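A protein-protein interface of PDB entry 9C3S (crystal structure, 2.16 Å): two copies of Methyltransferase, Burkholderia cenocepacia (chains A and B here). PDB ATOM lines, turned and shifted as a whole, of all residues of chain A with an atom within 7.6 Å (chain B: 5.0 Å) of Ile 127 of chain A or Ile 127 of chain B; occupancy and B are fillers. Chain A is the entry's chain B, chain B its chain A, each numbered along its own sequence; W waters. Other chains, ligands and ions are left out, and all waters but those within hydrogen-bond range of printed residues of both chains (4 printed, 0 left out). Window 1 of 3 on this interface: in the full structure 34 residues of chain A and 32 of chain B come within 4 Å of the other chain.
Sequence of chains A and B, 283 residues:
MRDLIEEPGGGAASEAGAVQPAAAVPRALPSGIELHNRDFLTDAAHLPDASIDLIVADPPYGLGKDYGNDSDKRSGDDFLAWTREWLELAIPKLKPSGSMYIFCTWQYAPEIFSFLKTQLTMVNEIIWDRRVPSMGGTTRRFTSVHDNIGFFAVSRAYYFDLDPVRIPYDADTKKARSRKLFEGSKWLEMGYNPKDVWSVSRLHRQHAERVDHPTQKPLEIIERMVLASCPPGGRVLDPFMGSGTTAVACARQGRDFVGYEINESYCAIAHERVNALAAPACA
The side-chain carboxylate (OE1) of Glu 125 of chain B sits at hydrogen-bond distance from a ring nitrogen (NE2) of His 146 of chain A (2.7 Å). The side-chain carboxylate (OE1) of Glu 125 of chain B is in hydrogen-bond range of the side-chain amide nitrogen (ND2) of Asn 148 of chain A (3.1 Å). NE2 of His 146 of chain B is in hydrogen-bond range of OE1 of Glu 125 of chain A, at 2.7 Å. ND1 of His 146 of chain B lies within hydrogen-bond range of OD1 of Asp 196 of chain A (3.3 Å). The side-chain carboxylate of Glu 125 of chain A sits close to the side-chain amide oxygen of Asn 148 of chain B (3.1 Å). The side-chain carboxylate of Asp 196 of chain B sits at hydrogen-bond distance from the backbone NH of Val 145 of chain A (2.9 Å). The side-chain carboxylate of Asp 196 of chain B sits at hydrogen-bond distance from a ring nitrogen (ND1) of His 146 of chain A (3.1 Å).
The side-chain carboxylate of Glu 125 of chain B sits at hydrogen-bond distance from the side-chain amide nitrogen of Asn 148 of chain B, at 3.0 Å. The backbone NH (N) of Arg 130 of chain A lies within hydrogen-bond range of the backbone carbonyl oxygen (O) of Val 145 of chain A, at 2.8 Å.
Among the printed residues, merely in contact across the chains: Trp 106 of chain A with Glu 125 of chain B (3.4 Å), Glu 125 of chain A with Glu 125 of chain B (3.7 Å), Ile 127 of chain A with Ile 127 of chain B (3.5 Å), Ile 127 of chain A with His 146 of chain B (3.6 Å), Val 145 of chain A with Val 197 of chain B (3.4 Å), His 146 of chain A with Ile 127 of chain B (3.5 Å), His 146 of chain A with Val 197 of chain B (3.5 Å) and Val 197 of chain A with His 146 of chain B (3.5 Å).
Of chain B, only Ile 127 (3.5 Å) and His 146 (3.6 Å) come within 4 Å of Ile 127 of chain A. Of the printed residues of chain B, Val 145 of chain A touches Asp 196 (2.9 Å) and Val 197 (3.4 Å). Of the printed residues of chain A, Ile 127 of chain B touches Ile 127 (3.5 Å) and His 146 (3.5 Å). Asp 147 of chain B touches none of the printed residues of chain A. The nearest residue of chain B that does not touch Ile 127 of chain A is Val 197 of chain B (4.8 Å). The nearest residue of chain A that does not touch Ile 127 of chain B is Val 197 of chain A (4.7 Å).
Of the 22 printed residues of chain A, 8 touch a printed residue of chain B. Hydrophobic or aromatic side chains of chain A within 4 Å of the printed part of chain B: Trp 106, Ile 127, Val 145, His 146 and Val 197. Hydrophobic or aromatic side chains of chain B that line the printed part of chain A: Ile 127, His 146 and Val 197. Among the printed residues, no Asp or Glu carboxylate lies within 4 Å of a Lys or Arg side-chain nitrogen of the other chain.
Ile 127 of chain A touches its own counterpart, Ile 127 of chain B. His 146 of chain A touches Val 197 of chain B, and with the chains exchanged Val 197 of chain A touches His 146 of chain B.
Water W4 lies within hydrogen-bond range of the side-chain hydroxyl of Ser 199 of chain A (2.9 Å) and the side-chain carboxylate of Asp 129 of chain B (3.0 Å).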
ATOM      1  N   TRP A 106     -14.678 -19.170   3.582  1.00  0.00           N
ATOM      2  CA  TRP A 106     -15.387 -18.368   2.595  1.00  0.00           C
ATOM      3  C   TRP A 106     -16.305 -19.223   1.733  1.00  0.00           C
ATOM      4  O   TRP A 106     -17.307 -18.726   1.209  1.00  0.00           O
ATOM      5  CB  TRP A 106     -14.381 -17.619   1.721  1.00  0.00           C
ATOM      6  CG  TRP A 106     -13.418 -18.527   1.036  1.00  0.00           C
ATOM      7  CD1 TRP A 106     -12.254 -19.021   1.546  1.00  0.00           C
ATOM      8  CD2 TRP A 106     -13.538 -19.063  -0.284  1.00  0.00           C
ATOM      9  NE1 TRP A 106     -11.640 -19.830   0.623  1.00  0.00           N
ATOM     10  CE2 TRP A 106     -12.406 -19.869  -0.511  1.00  0.00           C
ATOM     11  CE3 TRP A 106     -14.490 -18.935  -1.299  1.00  0.00           C
ATOM     12  CZ2 TRP A 106     -12.201 -20.546  -1.710  1.00  0.00           C
ATOM     13  CZ3 TRP A 106     -14.285 -19.606  -2.490  1.00  0.00           C
ATOM     14  CH2 TRP A 106     -13.149 -20.402  -2.686  1.00  0.00           C
ATOM     15  N   PHE A 113     -23.543 -16.613   7.215  1.00  0.00           N
ATOM     16  CA  PHE A 113     -23.780 -15.261   7.708  1.00  0.00           C
ATOM     17  C   PHE A 113     -25.137 -14.735   7.260  1.00  0.00           C
ATOM     18  O   PHE A 113     -25.798 -14.010   8.015  1.00  0.00           O
ATOM     19  CB  PHE A 113     -22.660 -14.332   7.242  1.00  0.00           C
ATOM     20  CG  PHE A 113     -21.308 -14.658   7.828  1.00  0.00           C
ATOM     21  CD1 PHE A 113     -21.158 -15.663   8.772  1.00  0.00           C
ATOM     22  CD2 PHE A 113     -20.187 -13.951   7.431  1.00  0.00           C
ATOM     23  CE1 PHE A 113     -19.916 -15.951   9.307  1.00  0.00           C
ATOM     24  CE2 PHE A 113     -18.943 -14.237   7.961  1.00  0.00           C
ATOM     25  CZ  PHE A 113     -18.808 -15.241   8.897  1.00  0.00           C
ATOM     26  N   ASN A 124     -19.526  -7.516  13.420  1.00  0.00           N
ATOM     27  CA  ASN A 124     -18.267  -7.452  12.687  1.00  0.00           C
ATOM     28  C   ASN A 124     -18.073  -8.714  11.862  1.00  0.00           C
ATOM     29  O   ASN A 124     -18.579  -9.786  12.199  1.00  0.00           O
ATOM     30  CB  ASN A 124     -17.057  -7.291  13.620  1.00  0.00           C
ATOM     31  CG  ASN A 124     -16.617  -5.847  13.785  1.00  0.00           C
ATOM     32  OD1 ASN A 124     -16.544  -5.339  14.906  1.00  0.00           O
ATOM     33  ND2 ASN A 124     -16.288  -5.187  12.676  1.00  0.00           N
ATOM     34  N   GLU A 125     -17.317  -8.572  10.779  1.00  0.00           N
ATOM     35  CA  GLU A 125     -16.737  -9.706  10.072  1.00  0.00           C
ATOM     36  C   GLU A 125     -15.232  -9.592  10.270  1.00  0.00           C
ATOM     37  O   GLU A 125     -14.576  -8.748   9.656  1.00  0.00           O
ATOM     38  CB  GLU A 125     -17.104  -9.726   8.592  1.00  0.00           C
ATOM     39  CG  GLU A 125     -16.572 -10.971   7.881  1.00  0.00           C
ATOM     40  CD  GLU A 125     -16.154 -10.725   6.441  1.00  0.00           C
ATOM     41  OE1 GLU A 125     -15.897  -9.557   6.076  1.00  0.00           O
ATOM     42  OE2 GLU A 125     -16.070 -11.714   5.677  1.00  0.00           O
ATOM     43  N   ILE A 126     -14.699 -10.428  11.146  1.00  0.00           N
ATOM     44  CA  ILE A 126     -13.281 -10.430  11.457  1.00  0.00           C
ATOM     45  C   ILE A 126     -12.594 -11.418  10.525  1.00  0.00           C
ATOM     46  O   ILE A 126     -13.077 -12.538  10.322  1.00  0.00           O
ATOM     47  CB  ILE A 126     -13.052 -10.786  12.935  1.00  0.00           C
ATOM     48  CG1 ILE A 126     -13.610  -9.673  13.828  1.00  0.00           C
ATOM     49  CG2 ILE A 126     -11.577 -10.992  13.226  1.00  0.00           C
ATOM     50  CD1 ILE A 126     -14.309 -10.172  15.072  1.00  0.00           C
ATOM     51  N   ILE A 127     -11.486 -10.995   9.929  1.00  0.00           N
ATOM     52  CA  ILE A 127     -10.699 -11.846   9.047  1.00  0.00           C
ATOM     53  C   ILE A 127      -9.468 -12.291   9.814  1.00  0.00           C
ATOM     54  O   ILE A 127      -8.638 -11.460  10.200  1.00  0.00           O
ATOM     55  CB  ILE A 127     -10.301 -11.108   7.759  1.00  0.00           C
ATOM     56  CG1 ILE A 127     -11.545 -10.674   6.986  1.00  0.00           C
ATOM     57  CG2 ILE A 127      -9.408 -11.990   6.897  1.00  0.00           C
ATOM     58  CD1 ILE A 127     -12.422 -11.834   6.527  1.00  0.00           C
ATOM     59  N   TRP A 128      -9.338 -13.594  10.047  1.00  0.00           N
ATOM     60  CA  TRP A 128      -8.108 -14.130  10.614  1.00  0.00           C
ATOM     61  C   TRP A 128      -7.141 -14.359   9.462  1.00  0.00           C
ATOM     62  O   TRP A 128      -7.355 -15.251   8.635  1.00  0.00           O
ATOM     63  CB  TRP A 128      -8.348 -15.424  11.386  1.00  0.00           C
ATOM     64  CG  TRP A 128      -7.057 -16.037  11.850  1.00  0.00           C
ATOM     65  CD1 TRP A 128      -5.903 -15.370  12.159  1.00  0.00           C
ATOM     66  CD2 TRP A 128      -6.779 -17.428  12.049  1.00  0.00           C
ATOM     67  NE1 TRP A 128      -4.928 -16.260  12.537  1.00  0.00           N
ATOM     68  CE2 TRP A 128      -5.441 -17.529  12.481  1.00  0.00           C
ATOM     69  CE3 TRP A 128      -7.532 -18.597  11.907  1.00  0.00           C
ATOM     70  CZ2 TRP A 128      -4.840 -18.751  12.773  1.00  0.00           C
ATOM     71  CZ3 TRP A 128      -6.933 -19.810  12.197  1.00  0.00           C
ATOM     72  CH2 TRP A 128      -5.601 -19.877  12.624  1.00  0.00           C
ATOM     73  N   ASP A 129      -6.094 -13.543   9.400  1.00  0.00           N
ATOM     74  CA  ASP A 129      -5.018 -13.706   8.424  1.00  0.00           C
ATOM     75  C   ASP A 129      -3.993 -14.654   9.028  1.00  0.00           C
ATOM     76  O   ASP A 129      -3.162 -14.255   9.846  1.00  0.00           O
ATOM     77  CB  ASP A 129      -4.398 -12.357   8.075  1.00  0.00           C
ATOM     78  CG  ASP A 129      -3.134 -12.491   7.240  1.00  0.00           C
ATOM     79  OD1 ASP A 129      -2.869 -13.599   6.727  1.00  0.00           O
ATOM     80  OD2 ASP A 129      -2.406 -11.484   7.098  1.00  0.00           O
ATOM     81  N   ARG A 130      -4.043 -15.918   8.611  1.00  0.00           N
ATOM     82  CA  ARG A 130      -3.196 -16.949   9.194  1.00  0.00           C
ATOM     83  C   ARG A 130      -1.723 -16.786   8.848  1.00  0.00           C
ATOM     84  O   ARG A 130      -0.897 -17.524   9.395  1.00  0.00           O
ATOM     85  CB  ARG A 130      -3.695 -18.323   8.742  1.00  0.00           C
ATOM     86  CG  ARG A 130      -5.117 -18.628   9.209  1.00  0.00           C
ATOM     87  CD  ARG A 130      -5.928 -19.414   8.181  1.00  0.00           C
ATOM     88  NE  ARG A 130      -5.107 -20.289   7.352  1.00  0.00           N
ATOM     89  CZ  ARG A 130      -5.539 -20.897   6.255  1.00  0.00           C
ATOM     90  NH1 ARG A 130      -6.773 -20.731   5.812  1.00  0.00           N
ATOM     91  NH2 ARG A 130      -4.709 -21.690   5.583  1.00  0.00           N
ATOM     92  N   VAL A 145      -5.301 -18.053   2.806  1.00  0.00           N
ATOM     93  CA  VAL A 145      -4.484 -17.595   3.921  1.00  0.00           C
ATOM     94  C   VAL A 145      -5.339 -16.909   4.978  1.00  0.00           C
ATOM     95  O   VAL A 145      -4.803 -16.334   5.934  1.00  0.00           O
ATOM     96  CB  VAL A 145      -3.361 -16.661   3.434  1.00  0.00           C
ATOM     97  CG1 VAL A 145      -3.882 -15.252   3.192  1.00  0.00           C
ATOM     98  CG2 VAL A 145      -2.229 -16.635   4.436  1.00  0.00           C
ATOM     99  N   HIS A 146      -6.664 -16.966   4.838  1.00  0.00           N
ATOM    100  CA  HIS A 146      -7.532 -16.361   5.838  1.00  0.00           C
ATOM    101  C   HIS A 146      -8.725 -17.256   6.136  1.00  0.00           C
ATOM    102  O   HIS A 146      -9.181 -18.031   5.292  1.00  0.00           O
ATOM    103  CB  HIS A 146      -8.029 -14.971   5.408  1.00  0.00           C
ATOM    104  CG  HIS A 146      -9.223 -14.995   4.506  1.00  0.00           C
ATOM    105  ND1 HIS A 146      -9.136 -15.285   3.161  1.00  0.00           N
ATOM    106  CD2 HIS A 146     -10.531 -14.743   4.751  1.00  0.00           C
ATOM    107  CE1 HIS A 146     -10.340 -15.222   2.618  1.00  0.00           C
ATOM    108  NE2 HIS A 146     -11.205 -14.895   3.562  1.00  0.00           N
ATOM    109  N   ASP A 147      -9.210 -17.133   7.367  1.00  0.00           N
ATOM    110  CA  ASP A 147     -10.457 -17.740   7.809  1.00  0.00           C
ATOM    111  C   ASP A 147     -11.417 -16.626   8.206  1.00  0.00           C
ATOM    112  O   ASP A 147     -10.988 -15.521   8.564  1.00  0.00           O
ATOM    113  CB  ASP A 147     -10.235 -18.695   8.991  1.00  0.00           C
ATOM    114  CG  ASP A 147      -9.383 -19.895   8.620  1.00  0.00           C
ATOM    115  OD1 ASP A 147      -9.057 -20.050   7.424  1.00  0.00           O
ATOM    116  OD2 ASP A 147      -9.040 -20.683   9.530  1.00  0.00           O
ATOM    117  N   ASN A 148     -12.718 -16.907   8.135  1.00  0.00           N
ATOM    118  CA  ASN A 148     -13.733 -15.897   8.398  1.00  0.00           C
ATOM    119  C   ASN A 148     -14.322 -16.103   9.784  1.00  0.00           C
ATOM    120  O   ASN A 148     -14.533 -17.240  10.214  1.00  0.00           O
ATOM    121  CB  ASN A 148     -14.843 -15.956   7.347  1.00  0.00           C
ATOM    122  CG  ASN A 148     -14.329 -15.696   5.944  1.00  0.00           C
ATOM    123  OD1 ASN A 148     -13.533 -16.469   5.411  1.00  0.00           O
ATOM    124  ND2 ASN A 148     -14.775 -14.596   5.341  1.00  0.00           N
ATOM    125  N   ILE A 149     -14.595 -14.999  10.481  1.00  0.00           N
ATOM    126  CA  ILE A 149     -15.230 -15.037  11.792  1.00  0.00           C
ATOM    127  C   ILE A 149     -16.391 -14.057  11.778  1.00  0.00           C
ATOM    128  O   ILE A 149     -16.192 -12.852  11.582  1.00  0.00           O
ATOM    129  CB  ILE A 149     -14.257 -14.685  12.927  1.00  0.00           C
ATOM    130  CG1 ILE A 149     -13.005 -15.559  12.862  1.00  0.00           C
ATOM    131  CG2 ILE A 149     -14.940 -14.857  14.275  1.00  0.00           C
ATOM    132  CD1 ILE A 149     -11.897 -15.054  13.744  1.00  0.00           C
ATOM    133  N   GLY A 150     -17.600 -14.569  11.990  1.00  0.00           N
ATOM    134  CA  GLY A 150     -18.758 -13.718  12.168  1.00  0.00           C
ATOM    135  C   GLY A 150     -18.918 -13.375  13.634  1.00  0.00           C
ATOM    136  O   GLY A 150     -18.886 -14.261  14.494  1.00  0.00           O
ATOM    137  N   LYS A 195      -8.756  -4.069  15.284  1.00  0.00           N
ATOM    138  CA  LYS A 195      -9.299  -4.004  13.929  1.00  0.00           C
ATOM    139  C   LYS A 195      -9.948  -5.329  13.546  1.00  0.00           C
ATOM    140  O   LYS A 195      -9.810  -6.321  14.272  1.00  0.00           O
ATOM    141  CB  LYS A 195      -8.204  -3.616  12.928  1.00  0.00           C
ATOM    142  CG  LYS A 195      -7.652  -2.214  13.163  1.00  0.00           C
ATOM    143  CD  LYS A 195      -6.480  -1.881  12.242  1.00  0.00           C
ATOM    144  CE  LYS A 195      -5.255  -1.405  13.009  1.00  0.00           C
ATOM    145  NZ  LYS A 195      -4.257  -2.506  13.131  1.00  0.00           N
ATOM    146  N   ASP A 196     -10.672  -5.361  12.421  1.00  0.00           N
ATOM    147  CA  ASP A 196     -11.351  -6.571  11.980  1.00  0.00           C
ATOM    148  C   ASP A 196     -10.505  -7.405  11.021  1.00  0.00           C
ATOM    149  O   ASP A 196     -11.053  -8.210  10.261  1.00  0.00           O
ATOM    150  CB  ASP A 196     -12.703  -6.232  11.339  1.00  0.00           C
ATOM    151  CG  ASP A 196     -12.575  -5.388  10.086  1.00  0.00           C
ATOM    152  OD1 ASP A 196     -11.444  -5.215   9.584  1.00  0.00           O
ATOM    153  OD2 ASP A 196     -13.621  -4.912   9.589  1.00  0.00           O
ATOM    154  N   VAL A 197      -9.190  -7.221  11.031  1.00  0.00           N
ATOM    155  CA  VAL A 197      -8.256  -8.174  10.445  1.00  0.00           C
ATOM    156  C   VAL A 197      -7.215  -8.489  11.503  1.00  0.00           C
ATOM    157  O   VAL A 197      -6.544  -7.580  12.006  1.00  0.00           O
ATOM    158  CB  VAL A 197      -7.572  -7.643   9.176  1.00  0.00           C
ATOM    159  CG1 VAL A 197      -6.591  -8.679   8.667  1.00  0.00           C
ATOM    160  CG2 VAL A 197      -8.592  -7.322   8.111  1.00  0.00           C
ATOM    161  N   TRP A 198      -7.078  -9.769  11.839  1.00  0.00           N
ATOM    162  CA  TRP A 198      -6.147 -10.223  12.866  1.00  0.00           C
ATOM    163  C   TRP A 198      -5.055 -11.052  12.203  1.00  0.00           C
ATOM    164  O   TRP A 198      -5.299 -12.193  11.792  1.00  0.00           O
ATOM    165  CB  TRP A 198      -6.877 -11.037  13.929  1.00  0.00           C
ATOM    166  CG  TRP A 198      -7.976 -10.292  14.611  1.00  0.00           C
ATOM    167  CD1 TRP A 198      -8.239  -8.955  14.536  1.00  0.00           C
ATOM    168  CD2 TRP A 198      -8.964 -10.847  15.482  1.00  0.00           C
ATOM    169  NE1 TRP A 198      -9.334  -8.645  15.307  1.00  0.00           N
ATOM    170  CE2 TRP A 198      -9.796  -9.791  15.898  1.00  0.00           C
ATOM    171  CE3 TRP A 198      -9.224 -12.135  15.952  1.00  0.00           C
ATOM    172  CZ2 TRP A 198     -10.870  -9.984  16.762  1.00  0.00           C
ATOM    173  CZ3 TRP A 198     -10.289 -12.328  16.808  1.00  0.00           C
ATOM    174  CH2 TRP A 198     -11.100 -11.258  17.204  1.00  0.00           C
ATOM    175  N   SER A 199      -3.849 -10.483  12.111  1.00  0.00           N
ATOM    176  CA  SER A 199      -2.721 -11.149  11.453  1.00  0.00           C
ATOM    177  C   SER A 199      -1.908 -11.901  12.502  1.00  0.00           C
ATOM    178  O   SER A 199      -0.864 -11.449  12.978  1.00  0.00           O
ATOM    179  CB  SER A 199      -1.865 -10.139  10.699  1.00  0.00           C
ATOM    180  OG  SER A 199      -2.661  -9.109  10.136  1.00  0.00           O
ATOM    181  N   VAL A 200      -2.402 -13.082  12.858  1.00  0.00           N
ATOM    182  CA  VAL A 200      -1.762 -13.953  13.837  1.00  0.00           C
ATOM    183  C   VAL A 200      -1.422 -15.256  13.132  1.00  0.00           C
ATOM    184  O   VAL A 200      -2.313 -15.929  12.599  1.00  0.00           O
ATOM    185  CB  VAL A 200      -2.662 -14.203  15.054  1.00  0.00           C
ATOM    186  CG1 VAL A 200      -1.841 -14.714  16.230  1.00  0.00           C
ATOM    187  CG2 VAL A 200      -3.408 -12.927  15.422  1.00  0.00           C
ATOM    188  N   ILE A 221      -6.043 -15.110  19.639  1.00  0.00           N
ATOM    189  CA  ILE A 221      -7.301 -14.578  19.123  1.00  0.00           C
ATOM    190  C   ILE A 221      -8.471 -14.997  20.010  1.00  0.00           C
ATOM    191  O   ILE A 221      -9.383 -14.199  20.274  1.00  0.00           O
ATOM    192  CB  ILE A 221      -7.499 -15.019  17.658  1.00  0.00           C
ATOM    193  CG1 ILE A 221      -7.503 -16.546  17.533  1.00  0.00           C
ATOM    194  CG2 ILE A 221      -6.396 -14.442  16.773  1.00  0.00           C
ATOM    195  CD1 ILE A 221      -7.885 -17.046  16.151  1.00  0.00           C
ATOM    196  N   GLU B 125     -12.504 -15.709  -2.324  1.00  0.00           N
ATOM    197  CA  GLU B 125     -12.814 -14.496  -1.581  1.00  0.00           C
ATOM    198  C   GLU B 125     -11.480 -13.841  -1.267  1.00  0.00           C
ATOM    199  O   GLU B 125     -10.712 -14.346  -0.441  1.00  0.00           O
ATOM    200  CB  GLU B 125     -13.594 -14.768  -0.300  1.00  0.00           C
ATOM    201  CG  GLU B 125     -14.091 -13.477   0.350  1.00  0.00           C
ATOM    202  CD  GLU B 125     -14.378 -13.621   1.832  1.00  0.00           C
ATOM    203  OE1 GLU B 125     -13.648 -14.374   2.513  1.00  0.00           O
ATOM    204  OE2 GLU B 125     -15.330 -12.971   2.315  1.00  0.00           O
ATOM    205  N   ILE B 126     -11.202 -12.739  -1.944  1.00  0.00           N
ATOM    206  CA  ILE B 126     -10.004 -11.955  -1.707  1.00  0.00           C
ATOM    207  C   ILE B 126     -10.331 -10.896  -0.664  1.00  0.00           C
ATOM    208  O   ILE B 126     -11.382 -10.248  -0.725  1.00  0.00           O
ATOM    209  CB  ILE B 126      -9.507 -11.325  -3.019  1.00  0.00           C
ATOM    210  CG1 ILE B 126      -8.929 -12.410  -3.934  1.00  0.00           C
ATOM    211  CG2 ILE B 126      -8.480 -10.258  -2.746  1.00  0.00           C
ATOM    212  CD1 ILE B 126      -9.644 -12.523  -5.258  1.00  0.00           C
ATOM    213  N   ILE B 127      -9.466 -10.735   0.322  1.00  0.00           N
ATOM    214  CA  ILE B 127      -9.646  -9.729   1.404  1.00  0.00           C
ATOM    215  C   ILE B 127      -8.658  -8.595   1.134  1.00  0.00           C
ATOM    216  O   ILE B 127      -7.491  -8.816   1.336  1.00  0.00           O
ATOM    217  CB  ILE B 127      -9.417 -10.351   2.797  1.00  0.00           C
ATOM    218  CG1 ILE B 127     -10.369 -11.523   3.078  1.00  0.00           C
ATOM    219  CG2 ILE B 127      -9.489  -9.284   3.887  1.00  0.00           C
ATOM    220  CD1 ILE B 127     -11.841 -11.156   3.139  1.00  0.00           C
ATOM    221  N   TRP B 128      -9.123  -7.425   0.750  1.00  0.00           N
ATOM    222  CA  TRP B 128      -8.212  -6.271   0.620  1.00  0.00           C
ATOM    223  C   TRP B 128      -7.954  -5.709   2.017  1.00  0.00           C
ATOM    224  O   TRP B 128      -8.853  -5.091   2.563  1.00  0.00           O
ATOM    225  CB  TRP B 128      -8.754  -5.190  -0.318  1.00  0.00           C
ATOM    226  CG  TRP B 128      -7.882  -3.967  -0.395  1.00  0.00           C
ATOM    227  CD1 TRP B 128      -6.524  -3.914  -0.300  1.00  0.00           C
ATOM    228  CD2 TRP B 128      -8.323  -2.605  -0.564  1.00  0.00           C
ATOM    229  NE1 TRP B 128      -6.090  -2.624  -0.407  1.00  0.00           N
ATOM    230  CE2 TRP B 128      -7.167  -1.798  -0.567  1.00  0.00           C
ATOM    231  CE3 TRP B 128      -9.570  -1.994  -0.715  1.00  0.00           C
ATOM    232  CZ2 TRP B 128      -7.226  -0.417  -0.711  1.00  0.00           C
ATOM    233  CZ3 TRP B 128      -9.624  -0.628  -0.861  1.00  0.00           C
ATOM    234  CH2 TRP B 128      -8.469   0.148  -0.857  1.00  0.00           C
ATOM    235  N   ASP B 129      -6.763  -5.920   2.546  1.00  0.00           N
ATOM    236  CA  ASP B 129      -6.372  -5.362   3.861  1.00  0.00           C
ATOM    237  C   ASP B 129      -5.891  -3.937   3.604  1.00  0.00           C
ATOM    238  O   ASP B 129      -4.786  -3.791   3.128  1.00  0.00           O
ATOM    239  CB  ASP B 129      -5.371  -6.256   4.556  1.00  0.00           C
ATOM    240  CG  ASP B 129      -4.777  -5.663   5.822  1.00  0.00           C
ATOM    241  OD1 ASP B 129      -5.277  -4.614   6.258  1.00  0.00           O
ATOM    242  OD2 ASP B 129      -3.826  -6.257   6.354  1.00  0.00           O
ATOM    243  N   HIS B 146     -10.746  -3.776   6.183  1.00  0.00           N
ATOM    244  CA  HIS B 146     -10.733  -4.708   5.034  1.00  0.00           C
ATOM    245  C   HIS B 146     -11.961  -4.517   4.150  1.00  0.00           C
ATOM    246  O   HIS B 146     -13.002  -4.213   4.721  1.00  0.00           O
ATOM    247  CB  HIS B 146     -10.605  -6.155   5.523  1.00  0.00           C
ATOM    248  CG  HIS B 146     -11.876  -6.861   5.775  1.00  0.00           C
ATOM    249  ND1 HIS B 146     -12.583  -6.761   6.950  1.00  0.00           N
ATOM    250  CD2 HIS B 146     -12.555  -7.693   4.997  1.00  0.00           C
ATOM    251  CE1 HIS B 146     -13.665  -7.508   6.857  1.00  0.00           C
ATOM    252  NE2 HIS B 146     -13.658  -8.087   5.687  1.00  0.00           N
ATOM    253  N   ASP B 147     -11.802  -4.610   2.836  1.00  0.00           N
ATOM    254  CA  ASP B 147     -12.930  -4.605   1.871  1.00  0.00           C
ATOM    255  C   ASP B 147     -12.994  -6.038   1.358  1.00  0.00           C
ATOM    256  O   ASP B 147     -11.927  -6.658   1.247  1.00  0.00           O
ATOM    257  CB  ASP B 147     -12.761  -3.614   0.732  1.00  0.00           C
ATOM    258  CG  ASP B 147     -12.867  -2.138   1.076  1.00  0.00           C
ATOM    259  OD1 ASP B 147     -13.225  -1.831   2.210  1.00  0.00           O
ATOM    260  OD2 ASP B 147     -12.594  -1.308   0.198  1.00  0.00           O
ATOM    261  N   ASN B 148     -14.185  -6.545   1.086  1.00  0.00           N
ATOM    262  CA  ASN B 148     -14.378  -7.927   0.583  1.00  0.00           C
ATOM    263  C   ASN B 148     -14.365  -7.892  -0.945  1.00  0.00           C
ATOM    264  O   ASN B 148     -14.896  -6.915  -1.485  1.00  0.00           O
ATOM    265  CB  ASN B 148     -15.655  -8.539   1.138  1.00  0.00           C
ATOM    266  CG  ASN B 148     -15.572  -8.811   2.619  1.00  0.00           C
ATOM    267  OD1 ASN B 148     -15.867  -7.929   3.429  1.00  0.00           O
ATOM    268  ND2 ASN B 148     -15.187 -10.020   2.995  1.00  0.00           N
ATOM    269  N   ASP B 196      -5.128 -15.090  -0.817  1.00  0.00           N
ATOM    270  CA  ASP B 196      -6.432 -14.442  -0.846  1.00  0.00           C
ATOM    271  C   ASP B 196      -6.557 -13.314   0.175  1.00  0.00           C
ATOM    272  O   ASP B 196      -7.673 -12.878   0.470  1.00  0.00           O
ATOM    273  CB  ASP B 196      -7.553 -15.467  -0.629  1.00  0.00           C
ATOM    274  CG  ASP B 196      -7.407 -16.239   0.666  1.00  0.00           C
ATOM    275  OD1 ASP B 196      -6.591 -15.833   1.518  1.00  0.00           O
ATOM    276  OD2 ASP B 196      -8.128 -17.246   0.839  1.00  0.00           O
ATOM    277  N   VAL B 197      -5.446 -12.839   0.728  1.00  0.00           N
ATOM    278  CA  VAL B 197      -5.419 -11.578   1.459  1.00  0.00           C
ATOM    279  C   VAL B 197      -4.343 -10.708   0.833  1.00  0.00           C
ATOM    280  O   VAL B 197      -3.162 -11.079   0.835  1.00  0.00           O
ATOM    281  CB  VAL B 197      -5.150 -11.761   2.960  1.00  0.00           C
ATOM    282  CG1 VAL B 197      -5.281 -10.420   3.671  1.00  0.00           C
ATOM    283  CG2 VAL B 197      -6.109 -12.757   3.549  1.00  0.00           C
ATOM    284  N   TRP B 198      -4.749  -9.557   0.305  1.00  0.00           N
ATOM    285  CA  TRP B 198      -3.852  -8.595  -0.322  1.00  0.00           C
ATOM    286  C   TRP B 198      -3.698  -7.410   0.621  1.00  0.00           C
ATOM    287  O   TRP B 198      -4.630  -6.614   0.779  1.00  0.00           O
ATOM    288  CB  TRP B 198      -4.402  -8.147  -1.673  1.00  0.00           C
ATOM    289  CG  TRP B 198      -4.656  -9.271  -2.636  1.00  0.00           C
ATOM    290  CD1 TRP B 198      -4.276 -10.574  -2.500  1.00  0.00           C
ATOM    291  CD2 TRP B 198      -5.338  -9.182  -3.892  1.00  0.00           C
ATOM    292  NE1 TRP B 198      -4.685 -11.301  -3.594  1.00  0.00           N
ATOM    293  CE2 TRP B 198      -5.338 -10.469  -4.461  1.00  0.00           C
ATOM    294  CE3 TRP B 198      -5.951  -8.139  -4.584  1.00  0.00           C
ATOM    295  CZ2 TRP B 198      -5.931 -10.738  -5.694  1.00  0.00           C
ATOM    296  CZ3 TRP B 198      -6.540  -8.407  -5.808  1.00  0.00           C
ATOM    297  CH2 TRP B 198      -6.525  -9.695  -6.350  1.00  0.00           C
HETATM  298  O   HOH W   1     -10.656 -17.442  -1.306  1.00  0.00           O
HETATM  299  O   HOH W   2     -18.204 -13.015   3.543  1.00  0.00           O
HETATM  300  O   HOH W   3      -9.518 -18.575   2.601  1.00  0.00           O
HETATM  301  O   HOH W   4      -2.389  -6.436   8.978  1.00  0.00           O
